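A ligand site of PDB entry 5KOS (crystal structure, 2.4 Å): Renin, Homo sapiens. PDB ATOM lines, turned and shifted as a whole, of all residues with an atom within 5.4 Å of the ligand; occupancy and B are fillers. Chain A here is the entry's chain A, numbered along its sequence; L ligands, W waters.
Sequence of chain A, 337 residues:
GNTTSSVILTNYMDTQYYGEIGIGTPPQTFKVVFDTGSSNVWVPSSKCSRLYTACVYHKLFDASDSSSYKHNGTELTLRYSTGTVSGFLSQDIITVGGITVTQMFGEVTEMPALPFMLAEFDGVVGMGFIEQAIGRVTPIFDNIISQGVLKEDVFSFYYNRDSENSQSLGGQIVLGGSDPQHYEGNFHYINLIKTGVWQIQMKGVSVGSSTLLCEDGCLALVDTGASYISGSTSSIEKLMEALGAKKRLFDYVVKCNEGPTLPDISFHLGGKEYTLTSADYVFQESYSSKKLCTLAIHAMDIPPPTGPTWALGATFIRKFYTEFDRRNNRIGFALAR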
ATOM      1  N   THR A  15       9.432  18.253 -18.769  1.00  0.00           N
ATOM      2  CA  THR A  15      10.197  17.078 -19.200  1.00  0.00           C
ATOM      3  C   THR A  15      11.235  16.602 -18.190  1.00  0.00           C
ATOM      4  O   THR A  15      11.600  15.431 -18.205  1.00  0.00           O
ATOM      5  CB  THR A  15      10.916  17.351 -20.521  1.00  0.00           C
ATOM      6  OG1 THR A  15      11.805  18.467 -20.367  1.00  0.00           O
ATOM      7  CG2 THR A  15       9.912  17.672 -21.603  1.00  0.00           C
ATOM      8  N   GLN A  16      11.724  17.496 -17.320  1.00  0.00           N
ATOM      9  CA  GLN A  16      12.697  17.129 -16.324  1.00  0.00           C
ATOM     10  C   GLN A  16      12.260  17.675 -14.980  1.00  0.00           C
ATOM     11  O   GLN A  16      11.998  18.873 -14.848  1.00  0.00           O
ATOM     12  CB  GLN A  16      14.080  17.641 -16.711  1.00  0.00           C
ATOM     13  CG  GLN A  16      14.513  17.221 -18.113  1.00  0.00           C
ATOM     14  CD  GLN A  16      15.936  17.615 -18.460  1.00  0.00           C
ATOM     15  OE1 GLN A  16      16.816  17.644 -17.612  1.00  0.00           O
ATOM     16  NE2 GLN A  16      16.166  17.912 -19.717  1.00  0.00           N
ATOM     17  N   TYR A  17      12.142  16.784 -13.998  1.00  0.00           N
ATOM     18  CA  TYR A  17      11.848  17.155 -12.620  1.00  0.00           C
ATOM     19  C   TYR A  17      13.032  16.724 -11.763  1.00  0.00           C
ATOM     20  O   TYR A  17      13.469  15.580 -11.853  1.00  0.00           O
ATOM     21  CB  TYR A  17      10.578  16.480 -12.136  1.00  0.00           C
ATOM     22  CG  TYR A  17       9.329  16.954 -12.821  1.00  0.00           C
ATOM     23  CD1 TYR A  17       8.965  16.477 -14.068  1.00  0.00           C
ATOM     24  CD2 TYR A  17       8.491  17.889 -12.201  1.00  0.00           C
ATOM     25  CE1 TYR A  17       7.810  16.908 -14.690  1.00  0.00           C
ATOM     26  CE2 TYR A  17       7.338  18.327 -12.812  1.00  0.00           C
ATOM     27  CZ  TYR A  17       7.000  17.830 -14.048  1.00  0.00           C
ATOM     28  OH  TYR A  17       5.860  18.267 -14.641  1.00  0.00           O
ATOM     29  N   VAL A  33      17.637  13.928 -10.308  1.00  0.00           N
ATOM     30  CA  VAL A  33      16.350  13.290 -10.559  1.00  0.00           C
ATOM     31  C   VAL A  33      16.138  12.178  -9.525  1.00  0.00           C
ATOM     32  O   VAL A  33      17.043  11.394  -9.259  1.00  0.00           O
ATOM     33  CB  VAL A  33      16.279  12.706 -11.984  1.00  0.00           C
ATOM     34  CG1 VAL A  33      15.042  11.846 -12.188  1.00  0.00           C
ATOM     35  CG2 VAL A  33      16.307  13.839 -12.989  1.00  0.00           C
ATOM     36  N   ASP A  35      14.378   8.844  -8.980  1.00  0.00           N
ATOM     37  CA  ASP A  35      14.016   7.922 -10.055  1.00  0.00           C
ATOM     38  C   ASP A  35      13.560   6.578  -9.491  1.00  0.00           C
ATOM     39  O   ASP A  35      14.388   5.777  -9.062  1.00  0.00           O
ATOM     40  CB  ASP A  35      15.222   7.750 -10.979  1.00  0.00           C
ATOM     41  CG  ASP A  35      14.990   6.760 -12.090  1.00  0.00           C
ATOM     42  OD1 ASP A  35      13.815   6.463 -12.404  1.00  0.00           O
ATOM     43  OD2 ASP A  35      15.991   6.248 -12.654  1.00  0.00           O
ATOM     44  N   GLY A  37      12.491   4.154 -11.222  1.00  0.00           N
ATOM     45  CA  GLY A  37      12.913   3.128 -12.168  1.00  0.00           C
ATOM     46  C   GLY A  37      14.372   2.679 -12.087  1.00  0.00           C
ATOM     47  O   GLY A  37      14.796   1.886 -12.922  1.00  0.00           O
ATOM     48  N   SER A  38      15.160   3.212 -11.145  1.00  0.00           N
ATOM     49  CA  SER A  38      16.523   2.742 -10.897  1.00  0.00           C
ATOM     50  C   SER A  38      16.807   2.808  -9.400  1.00  0.00           C
ATOM     51  O   SER A  38      16.026   3.381  -8.626  1.00  0.00           O
ATOM     52  CB  SER A  38      17.533   3.579 -11.682  1.00  0.00           C
ATOM     53  OG  SER A  38      17.666   4.900 -11.151  1.00  0.00           O
ATOM     54  N   TRP A  42      24.058   8.418  -8.200  1.00  0.00           N
ATOM     55  CA  TRP A  42      25.269   8.868  -8.861  1.00  0.00           C
ATOM     56  C   TRP A  42      25.262  10.361  -9.132  1.00  0.00           C
ATOM     57  O   TRP A  42      24.196  10.980  -9.318  1.00  0.00           O
ATOM     58  CB  TRP A  42      25.576   8.074 -10.150  1.00  0.00           C
ATOM     59  CG  TRP A  42      24.617   8.302 -11.294  1.00  0.00           C
ATOM     60  CD1 TRP A  42      23.533   7.526 -11.634  1.00  0.00           C
ATOM     61  CD2 TRP A  42      24.664   9.350 -12.279  1.00  0.00           C
ATOM     62  NE1 TRP A  42      22.924   8.033 -12.755  1.00  0.00           N
ATOM     63  CE2 TRP A  42      23.589   9.150 -13.165  1.00  0.00           C
ATOM     64  CE3 TRP A  42      25.512  10.443 -12.487  1.00  0.00           C
ATOM     65  CZ2 TRP A  42      23.333  10.001 -14.231  1.00  0.00           C
ATOM     66  CZ3 TRP A  42      25.257  11.302 -13.540  1.00  0.00           C
ATOM     67  CH2 TRP A  42      24.172  11.073 -14.399  1.00  0.00           C
ATOM     68  N   ARG A  79      23.486   1.316 -16.935  1.00  0.00           N
ATOM     69  CA  ARG A  79      22.896   1.339 -18.276  1.00  0.00           C
ATOM     70  C   ARG A  79      21.427   1.748 -18.194  1.00  0.00           C
ATOM     71  O   ARG A  79      20.602   1.010 -17.677  1.00  0.00           O
ATOM     72  CB  ARG A  79      23.047  -0.038 -18.941  1.00  0.00           C
ATOM     73  CG  ARG A  79      24.488  -0.485 -19.139  1.00  0.00           C
ATOM     74  CD  ARG A  79      24.599  -2.002 -19.277  1.00  0.00           C
ATOM     75  NE  ARG A  79      25.976  -2.475 -19.360  1.00  0.00           N
ATOM     76  CZ  ARG A  79      26.773  -2.662 -18.304  1.00  0.00           C
ATOM     77  NH1 ARG A  79      26.327  -2.388 -17.087  1.00  0.00           N
ATOM     78  NH2 ARG A  79      28.002  -3.104 -18.469  1.00  0.00           N
ATOM     79  N   TYR A  80      21.126   2.954 -18.682  1.00  0.00           N
ATOM     80  CA  TYR A  80      19.753   3.411 -18.793  1.00  0.00           C
ATOM     81  C   TYR A  80      19.282   3.235 -20.235  1.00  0.00           C
ATOM     82  O   TYR A  80      20.065   2.872 -21.113  1.00  0.00           O
ATOM     83  CB  TYR A  80      19.640   4.861 -18.374  1.00  0.00           C
ATOM     84  CG  TYR A  80      20.041   5.115 -16.951  1.00  0.00           C
ATOM     85  CD1 TYR A  80      19.154   4.876 -15.907  1.00  0.00           C
ATOM     86  CD2 TYR A  80      21.308   5.600 -16.632  1.00  0.00           C
ATOM     87  CE1 TYR A  80      19.501   5.119 -14.599  1.00  0.00           C
ATOM     88  CE2 TYR A  80      21.668   5.843 -15.316  1.00  0.00           C
ATOM     89  CZ  TYR A  80      20.764   5.598 -14.301  1.00  0.00           C
ATOM     90  OH  TYR A  80      21.123   5.833 -12.997  1.00  0.00           O
ATOM     91  N   SER A  81      17.997   3.480 -20.453  1.00  0.00           N
ATOM     92  CA  SER A  81      17.379   3.392 -21.778  1.00  0.00           C
ATOM     93  C   SER A  81      18.002   4.343 -22.779  1.00  0.00           C
ATOM     94  O   SER A  81      18.201   3.967 -23.924  1.00  0.00           O
ATOM     95  CB  SER A  81      15.887   3.730 -21.673  1.00  0.00           C
ATOM     96  OG  SER A  81      15.218   2.911 -20.728  1.00  0.00           O
ATOM     97  N   THR A  82      18.260   5.583 -22.358  1.00  0.00           N
ATOM     98  CA  THR A  82      18.749   6.621 -23.277  1.00  0.00           C
ATOM     99  C   THR A  82      20.260   6.785 -23.304  1.00  0.00           C
ATOM    100  O   THR A  82      20.769   7.586 -24.087  1.00  0.00           O
ATOM    101  CB  THR A  82      18.121   8.005 -22.995  1.00  0.00           C
ATOM    102  OG1 THR A  82      18.735   8.609 -21.837  1.00  0.00           O
ATOM    103  CG2 THR A  82      16.613   7.898 -22.810  1.00  0.00           C
ATOM    104  N   PRO A 115      23.234  11.322 -24.148  1.00  0.00           N
ATOM    105  CA  PRO A 115      22.165  12.314 -23.983  1.00  0.00           C
ATOM    106  C   PRO A 115      22.438  13.407 -22.935  1.00  0.00           C
ATOM    107  O   PRO A 115      21.598  14.273 -22.728  1.00  0.00           O
ATOM    108  CB  PRO A 115      21.013  11.438 -23.508  1.00  0.00           C
ATOM    109  CG  PRO A 115      21.691  10.439 -22.631  1.00  0.00           C
ATOM    110  CD  PRO A 115      22.966  10.099 -23.375  1.00  0.00           C
ATOM    111  N   PHE A 116      23.584  13.367 -22.262  1.00  0.00           N
ATOM    112  CA  PHE A 116      23.668  14.067 -20.974  1.00  0.00           C
ATOM    113  C   PHE A 116      23.879  15.580 -21.033  1.00  0.00           C
ATOM    114  O   PHE A 116      23.577  16.263 -20.061  1.00  0.00           O
ATOM    115  CB  PHE A 116      24.625  13.371 -20.041  1.00  0.00           C
ATOM    116  CG  PHE A 116      24.085  12.080 -19.530  1.00  0.00           C
ATOM    117  CD1 PHE A 116      23.090  12.079 -18.546  1.00  0.00           C
ATOM    118  CD2 PHE A 116      24.517  10.863 -20.054  1.00  0.00           C
ATOM    119  CE1 PHE A 116      22.555  10.883 -18.080  1.00  0.00           C
ATOM    120  CE2 PHE A 116      23.992   9.668 -19.589  1.00  0.00           C
ATOM    121  CZ  PHE A 116      23.014   9.680 -18.608  1.00  0.00           C
ATOM    122  N   LEU A 118      21.835  17.287 -22.549  1.00  0.00           N
ATOM    123  CA  LEU A 118      20.450  17.751 -22.519  1.00  0.00           C
ATOM    124  C   LEU A 118      19.860  17.714 -21.119  1.00  0.00           C
ATOM    125  O   LEU A 118      18.724  18.131 -20.930  1.00  0.00           O
ATOM    126  CB  LEU A 118      19.585  16.905 -23.454  1.00  0.00           C
ATOM    127  CG  LEU A 118      20.116  16.687 -24.860  1.00  0.00           C
ATOM    128  CD1 LEU A 118      19.183  15.720 -25.581  1.00  0.00           C
ATOM    129  CD2 LEU A 118      20.246  17.993 -25.623  1.00  0.00           C
ATOM    130  N   ALA A 119      20.606  17.199 -20.149  1.00  0.00           N
ATOM    131  CA  ALA A 119      20.120  17.078 -18.771  1.00  0.00           C
ATOM    132  C   ALA A 119      20.338  18.375 -18.004  1.00  0.00           C
ATOM    133  O   ALA A 119      21.471  18.858 -17.925  1.00  0.00           O
ATOM    134  CB  ALA A 119      20.829  15.937 -18.067  1.00  0.00           C
ATOM    135  N   PHE A 121      19.656  18.351 -14.824  1.00  0.00           N
ATOM    136  CA  PHE A 121      20.130  17.748 -13.594  1.00  0.00           C
ATOM    137  C   PHE A 121      21.577  17.260 -13.749  1.00  0.00           C
ATOM    138  O   PHE A 121      22.051  17.024 -14.851  1.00  0.00           O
ATOM    139  CB  PHE A 121      19.209  16.592 -13.202  1.00  0.00           C
ATOM    140  CG  PHE A 121      19.101  15.509 -14.247  1.00  0.00           C
ATOM    141  CD1 PHE A 121      20.010  14.465 -14.277  1.00  0.00           C
ATOM    142  CD2 PHE A 121      18.093  15.533 -15.210  1.00  0.00           C
ATOM    143  CE1 PHE A 121      19.916  13.468 -15.235  1.00  0.00           C
ATOM    144  CE2 PHE A 121      17.995  14.547 -16.175  1.00  0.00           C
ATOM    145  CZ  PHE A 121      18.908  13.508 -16.184  1.00  0.00           C
ATOM    146  N   VAL A 124      21.412  11.364 -10.469  1.00  0.00           N
ATOM    147  CA  VAL A 124      20.227  10.579 -10.218  1.00  0.00           C
ATOM    148  C   VAL A 124      20.305  10.009  -8.820  1.00  0.00           C
ATOM    149  O   VAL A 124      21.355   9.510  -8.406  1.00  0.00           O
ATOM    150  CB  VAL A 124      20.149   9.394 -11.208  1.00  0.00           C
ATOM    151  CG1 VAL A 124      18.946   8.498 -10.892  1.00  0.00           C
ATOM    152  CG2 VAL A 124      20.074   9.910 -12.639  1.00  0.00           C
ATOM    153  N   TYR A 159       4.327  15.922  -9.139  1.00  0.00           N
ATOM    154  CA  TYR A 159       4.908  16.669 -10.266  1.00  0.00           C
ATOM    155  C   TYR A 159       3.872  17.685 -10.756  1.00  0.00           C
ATOM    156  O   TYR A 159       2.823  17.308 -11.276  1.00  0.00           O
ATOM    157  CB  TYR A 159       5.299  15.732 -11.426  1.00  0.00           C
ATOM    158  CG  TYR A 159       6.560  14.900 -11.238  1.00  0.00           C
ATOM    159  CD1 TYR A 159       7.437  15.092 -10.167  1.00  0.00           C
ATOM    160  CD2 TYR A 159       6.882  13.929 -12.168  1.00  0.00           C
ATOM    161  CE1 TYR A 159       8.581  14.330 -10.030  1.00  0.00           C
ATOM    162  CE2 TYR A 159       8.030  13.145 -12.026  1.00  0.00           C
ATOM    163  CZ  TYR A 159       8.873  13.354 -10.953  1.00  0.00           C
ATOM    164  OH  TYR A 159      10.040  12.600 -10.799  1.00  0.00           O
ATOM    165  N   LEU A 221       5.838  -0.136 -15.475  1.00  0.00           N
ATOM    166  CA  LEU A 221       6.777   0.400 -14.506  1.00  0.00           C
ATOM    167  C   LEU A 221       6.321   1.806 -14.179  1.00  0.00           C
ATOM    168  O   LEU A 221       5.975   2.553 -15.075  1.00  0.00           O
ATOM    169  CB  LEU A 221       8.185   0.406 -15.108  1.00  0.00           C
ATOM    170  CG  LEU A 221       9.331   0.667 -14.131  1.00  0.00           C
ATOM    171  CD1 LEU A 221       9.693  -0.581 -13.342  1.00  0.00           C
ATOM    172  CD2 LEU A 221      10.541   1.156 -14.911  1.00  0.00           C
ATOM    173  N   ASP A 223       7.685   5.030 -13.209  1.00  0.00           N
ATOM    174  CA  ASP A 223       9.053   5.529 -13.332  1.00  0.00           C
ATOM    175  C   ASP A 223       9.113   7.043 -13.174  1.00  0.00           C
ATOM    176  O   ASP A 223       8.938   7.788 -14.144  1.00  0.00           O
ATOM    177  CB  ASP A 223       9.645   5.097 -14.681  1.00  0.00           C
ATOM    178  CG  ASP A 223      11.139   5.451 -14.823  1.00  0.00           C
ATOM    179  OD1 ASP A 223      11.720   6.067 -13.907  1.00  0.00           O
ATOM    180  OD2 ASP A 223      11.759   5.107 -15.867  1.00  0.00           O
ATOM    181  N   THR A 224       9.384   7.493 -11.952  1.00  0.00           N
ATOM    182  CA  THR A 224       9.426   8.929 -11.648  1.00  0.00           C
ATOM    183  C   THR A 224      10.557   9.641 -12.362  1.00  0.00           C
ATOM    184  O   THR A 224      10.507  10.856 -12.490  1.00  0.00           O
ATOM    185  CB  THR A 224       9.571   9.194 -10.149  1.00  0.00           C
ATOM    186  OG1 THR A 224      10.751   8.537  -9.652  1.00  0.00           O
ATOM    187  CG2 THR A 224       8.317   8.694  -9.392  1.00  0.00           C
ATOM    188  N   GLY A 225      11.559   8.898 -12.826  1.00  0.00           N
ATOM    189  CA  GLY A 225      12.693   9.477 -13.547  1.00  0.00           C
ATOM    190  C   GLY A 225      12.547   9.616 -15.048  1.00  0.00           C
ATOM    191  O   GLY A 225      13.422  10.163 -15.690  1.00  0.00           O
ATOM    192  N   ALA A 226      11.441   9.115 -15.600  1.00  0.00           N
ATOM    193  CA  ALA A 226      11.143   9.215 -17.018  1.00  0.00           C
ATOM    194  C   ALA A 226      10.152  10.360 -17.283  1.00  0.00           C
ATOM    195  O   ALA A 226       9.246  10.613 -16.491  1.00  0.00           O
ATOM    196  CB  ALA A 226      10.589   7.896 -17.528  1.00  0.00           C
ATOM    197  N   SER A 227      10.360  11.056 -18.401  1.00  0.00           N
ATOM    198  CA  SER A 227       9.562  12.228 -18.761  1.00  0.00           C
ATOM    199  C   SER A 227       8.189  11.816 -19.271  1.00  0.00           C
ATOM    200  O   SER A 227       7.206  12.479 -18.985  1.00  0.00           O
ATOM    201  CB  SER A 227      10.263  13.027 -19.865  1.00  0.00           C
ATOM    202  OG  SER A 227      11.625  13.223 -19.587  1.00  0.00           O
ATOM    203  N   MET A 300      10.216   2.897 -26.020  1.00  0.00           N
ATOM    204  CA  MET A 300      11.386   2.643 -25.176  1.00  0.00           C
ATOM    205  C   MET A 300      11.355   1.151 -24.885  1.00  0.00           C
ATOM    206  O   MET A 300      10.552   0.688 -24.076  1.00  0.00           O
ATOM    207  CB  MET A 300      11.329   3.490 -23.886  1.00  0.00           C
ATOM    208  CG  MET A 300      12.686   3.949 -23.363  1.00  0.00           C
ATOM    209  SD  MET A 300      12.577   5.238 -22.085  1.00  0.00           S
ATOM    210  CE  MET A 300      12.099   4.302 -20.634  1.00  0.00           C
ATOM    211  N   ILE A 302      12.638  -2.054 -23.243  1.00  0.00           N
ATOM    212  CA  ILE A 302      13.328  -2.332 -21.991  1.00  0.00           C
ATOM    213  C   ILE A 302      13.599  -3.838 -21.956  1.00  0.00           C
ATOM    214  O   ILE A 302      12.658  -4.628 -22.072  1.00  0.00           O
ATOM    215  CB  ILE A 302      12.466  -1.866 -20.809  1.00  0.00           C
ATOM    216  CG1 ILE A 302      12.346  -0.330 -20.843  1.00  0.00           C
ATOM    217  CG2 ILE A 302      13.045  -2.354 -19.477  1.00  0.00           C
ATOM    218  CD1 ILE A 302      11.298   0.270 -19.934  1.00  0.00           C
ATOM    219  N   PRO A 303      14.868  -4.255 -21.811  1.00  0.00           N
ATOM    220  CA  PRO A 303      15.162  -5.687 -21.945  1.00  0.00           C
ATOM    221  C   PRO A 303      14.759  -6.462 -20.690  1.00  0.00           C
ATOM    222  O   PRO A 303      14.536  -5.848 -19.648  1.00  0.00           O
ATOM    223  CB  PRO A 303      16.672  -5.712 -22.138  1.00  0.00           C
ATOM    224  CG  PRO A 303      17.167  -4.539 -21.349  1.00  0.00           C
ATOM    225  CD  PRO A 303      16.064  -3.511 -21.358  1.00  0.00           C
ATOM    226  N   THR A 306      13.345  -6.837 -16.612  1.00  0.00           N
ATOM    227  CA  THR A 306      12.405  -5.752 -16.292  1.00  0.00           C
ATOM    228  C   THR A 306      11.282  -5.625 -17.321  1.00  0.00           C
ATOM    229  O   THR A 306      10.127  -5.399 -16.945  1.00  0.00           O
ATOM    230  CB  THR A 306      13.115  -4.380 -16.178  1.00  0.00           C
ATOM    231  OG1 THR A 306      14.244  -4.491 -15.306  1.00  0.00           O
ATOM    232  CG2 THR A 306      12.178  -3.319 -15.623  1.00  0.00           C
ATOM    233  N   ALA A 314       6.465  11.135 -16.039  1.00  0.00           N
ATOM    234  CA  ALA A 314       5.926  12.397 -15.542  1.00  0.00           C
ATOM    235  C   ALA A 314       4.609  12.780 -16.186  1.00  0.00           C
ATOM    236  O   ALA A 314       3.749  13.326 -15.513  1.00  0.00           O
ATOM    237  CB  ALA A 314       6.933  13.529 -15.698  1.00  0.00           C
HETATM  238  C1  LIG L   1      14.090  13.456 -15.793  1.00  0.00           C
HETATM  239  C2  LIG L   1      14.502  13.220 -17.236  1.00  0.00           C
HETATM  240  C3  LIG L   1      15.612  11.415 -18.490  1.00  0.00           C
HETATM  241  C4  LIG L   1      15.147   8.893 -18.291  1.00  0.00           C
HETATM  242  C5  LIG L   1      17.747   9.330 -16.422  1.00  0.00           C
HETATM  243  C6  LIG L   1      14.987   6.816 -17.005  1.00  0.00           C
HETATM  244  C7  LIG L   1      14.943   6.780 -15.478  1.00  0.00           C
HETATM  245  C8  LIG L   1      15.057   4.335 -15.418  1.00  0.00           C
HETATM  246  C9  LIG L   1      15.603   2.987 -17.426  1.00  0.00           C
HETATM  247  C10 LIG L   1      10.796  13.173 -14.284  1.00  0.00           C
HETATM  248  O1  LIG L   1      12.066  13.764 -14.543  1.00  0.00           O
HETATM  249  C11 LIG L   1      12.581  13.317 -15.782  1.00  0.00           C
HETATM  250  N1  LIG L   1      14.774  11.788 -17.470  1.00  0.00           N
HETATM  251  N2  LIG L   1      16.286  12.374 -19.145  1.00  0.00           N
HETATM  252  C12 LIG L   1      17.105  12.083 -20.133  1.00  0.00           C
HETATM  253  N3  LIG L   1      17.292  10.832 -20.520  1.00  0.00           N
HETATM  254  C13 LIG L   1      16.672   9.818 -19.953  1.00  0.00           C
HETATM  255  C14 LIG L   1      15.804  10.063 -18.888  1.00  0.00           C
HETATM  256  O2  LIG L   1      13.984   8.743 -18.568  1.00  0.00           O
HETATM  257  N4  LIG L   1      15.774   7.977 -17.489  1.00  0.00           N
HETATM  258  C15 LIG L   1      17.219   8.058 -17.118  1.00  0.00           C
HETATM  259  C16 LIG L   1      17.097   9.620 -15.077  1.00  0.00           C
HETATM  260  C17 LIG L   1      19.250   9.154 -16.244  1.00  0.00           C
HETATM  261  N5  LIG L   1      14.347   5.531 -14.954  1.00  0.00           N
HETATM  262  C18 LIG L   1      14.925   4.255 -16.945  1.00  0.00           C
HETATM  263  C19 LIG L   1      15.569   5.507 -17.585  1.00  0.00           C
HETATM  264  O3  LIG L   1      16.752   3.091 -17.796  1.00  0.00           O
HETATM  265  N6  LIG L   1      14.999   1.756 -17.464  1.00  0.00           N
HETATM  266  C20 LIG L   1      15.755   0.571 -17.947  1.00  0.00           C
HETATM  267  C21 LIG L   1      15.779  -0.479 -16.822  1.00  0.00           C
HETATM  268  O4  LIG L   1      14.449  -0.689 -16.324  1.00  0.00           O
HETATM  269  C22 LIG L   1      13.742   0.477 -15.868  1.00  0.00           C
HETATM  270  C23 LIG L   1      13.612   1.484 -17.038  1.00  0.00           C
HETATM  271  C24 LIG L   1      17.845  13.204 -20.824  1.00  0.00           C
HETATM  272  C25 LIG L   1      17.372  14.604 -20.389  1.00  0.00           C
HETATM  273  C26 LIG L   1      19.316  13.064 -20.421  1.00  0.00           C
HETATM  274  C27 LIG L   1      17.670  13.085 -22.339  1.00  0.00           C
HETATM  275  O   HOH W   1      13.795  12.950 -21.339  1.00  0.00           O
HETATM  276  O   HOH W   2      12.471  10.398 -20.269  1.00  0.00           O
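A nitrogen (N1) of the ligand lies within hydrogen-bond range of the backbone carbonyl oxygen (O) of Gly 225 (2.8 Å). OD1 of Asp 35 is in salt-bridge range of N5 of the ligand (2.8 Å). The side-chain carboxylate (OD2) of Asp 223 is in salt-bridge range of a nitrogen (N5) of the ligand, 2.8 Å away. The side-chain hydroxyl (OG1) of Thr 82 is in hydrogen-bond range of a nitrogen (N3) of the ligand (3.0 Å). The backbone NH (N) of Ser 81 is in hydrogen-bond range of an oxygen (O3) of the ligand (3.0 Å). An oxygen (O3) of the ligand is in hydrogen-bond range of the side-chain hydroxyl (OG) of Ser 81 (3.3 Å). The backbone NH of Tyr 17 lies within hydrogen-bond range of an oxygen (O1) of the ligand.
Water W2 bridges an oxygen (O2) of the ligand (2.8 Å) and the backbone NH of Ser 227 (2.9 Å). Water W1 bridges the side-chain hydroxyl of Ser 227 (2.8 Å) and a nitrogen (N2) of the ligand (3.4 Å).
N of Gly 225 is in hydrogen-bond range of OD1 of Asp 35, at 3.3 Å. OD1 of Asp 223 is in hydrogen-bond range of N of Gly 225 (3.0 Å). OD1 of Asp 35 lies within hydrogen-bond range of N of Gly 37, at 2.9 Å. The side-chain carboxylate of Asp 35 is in hydrogen-bond range of the side-chain hydroxyl of Ser 38 (2.6 Å). O of Thr 224 sits at hydrogen-bond distance from OH of Tyr 159 (2.5 Å). The backbone carbonyl oxygen (O) of Ala 226 sits at hydrogen-bond distance from the backbone NH (N) of Ala 314. The backbone carbonyl oxygen (O) of Thr 15 is in hydrogen-bond range of the side-chain hydroxyl (OG) of Ser 227 (2.6 Å). NE2 of Gln 16 is in hydrogen-bond range of O of Leu 118.
Thr 15 touches the ligand. NE2 of Gln 16 touches C25 of the ligand, at 3.6 Å. Val 33 touches the ligand. Gly 37 touches the ligand (O to C22, 3.4 Å). CA of Tyr 80 touches O3 of the ligand (3.2 Å). O of Pro 115 touches C26 of the ligand, 3.5 Å away. Leu 118 touches the ligand. Phe 121 touches the ligand. Val 124 touches the ligand (CG2 to C17, 3.8 Å). Tyr 159 touches the ligand. Leu 221 touches the ligand. Thr 224 touches the ligand (O to C10, 2.9 Å). Ala 226 touches the ligand. Ser 227 touches the ligand. Ile 302 touches the ligand. CG2 of Thr 306 touches O4 of the ligand, at 3.5 Å. Hydrophobic or aromatic side chains within 4 Å of the ligand: Tyr 17, Val 33, Tyr 80, Pro 115, Phe 121, Val 124, Tyr 159, Leu 221, Ala 226 and Ile 302. Of the 30 residues printed, 22 come within 4 Å of the ligand.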
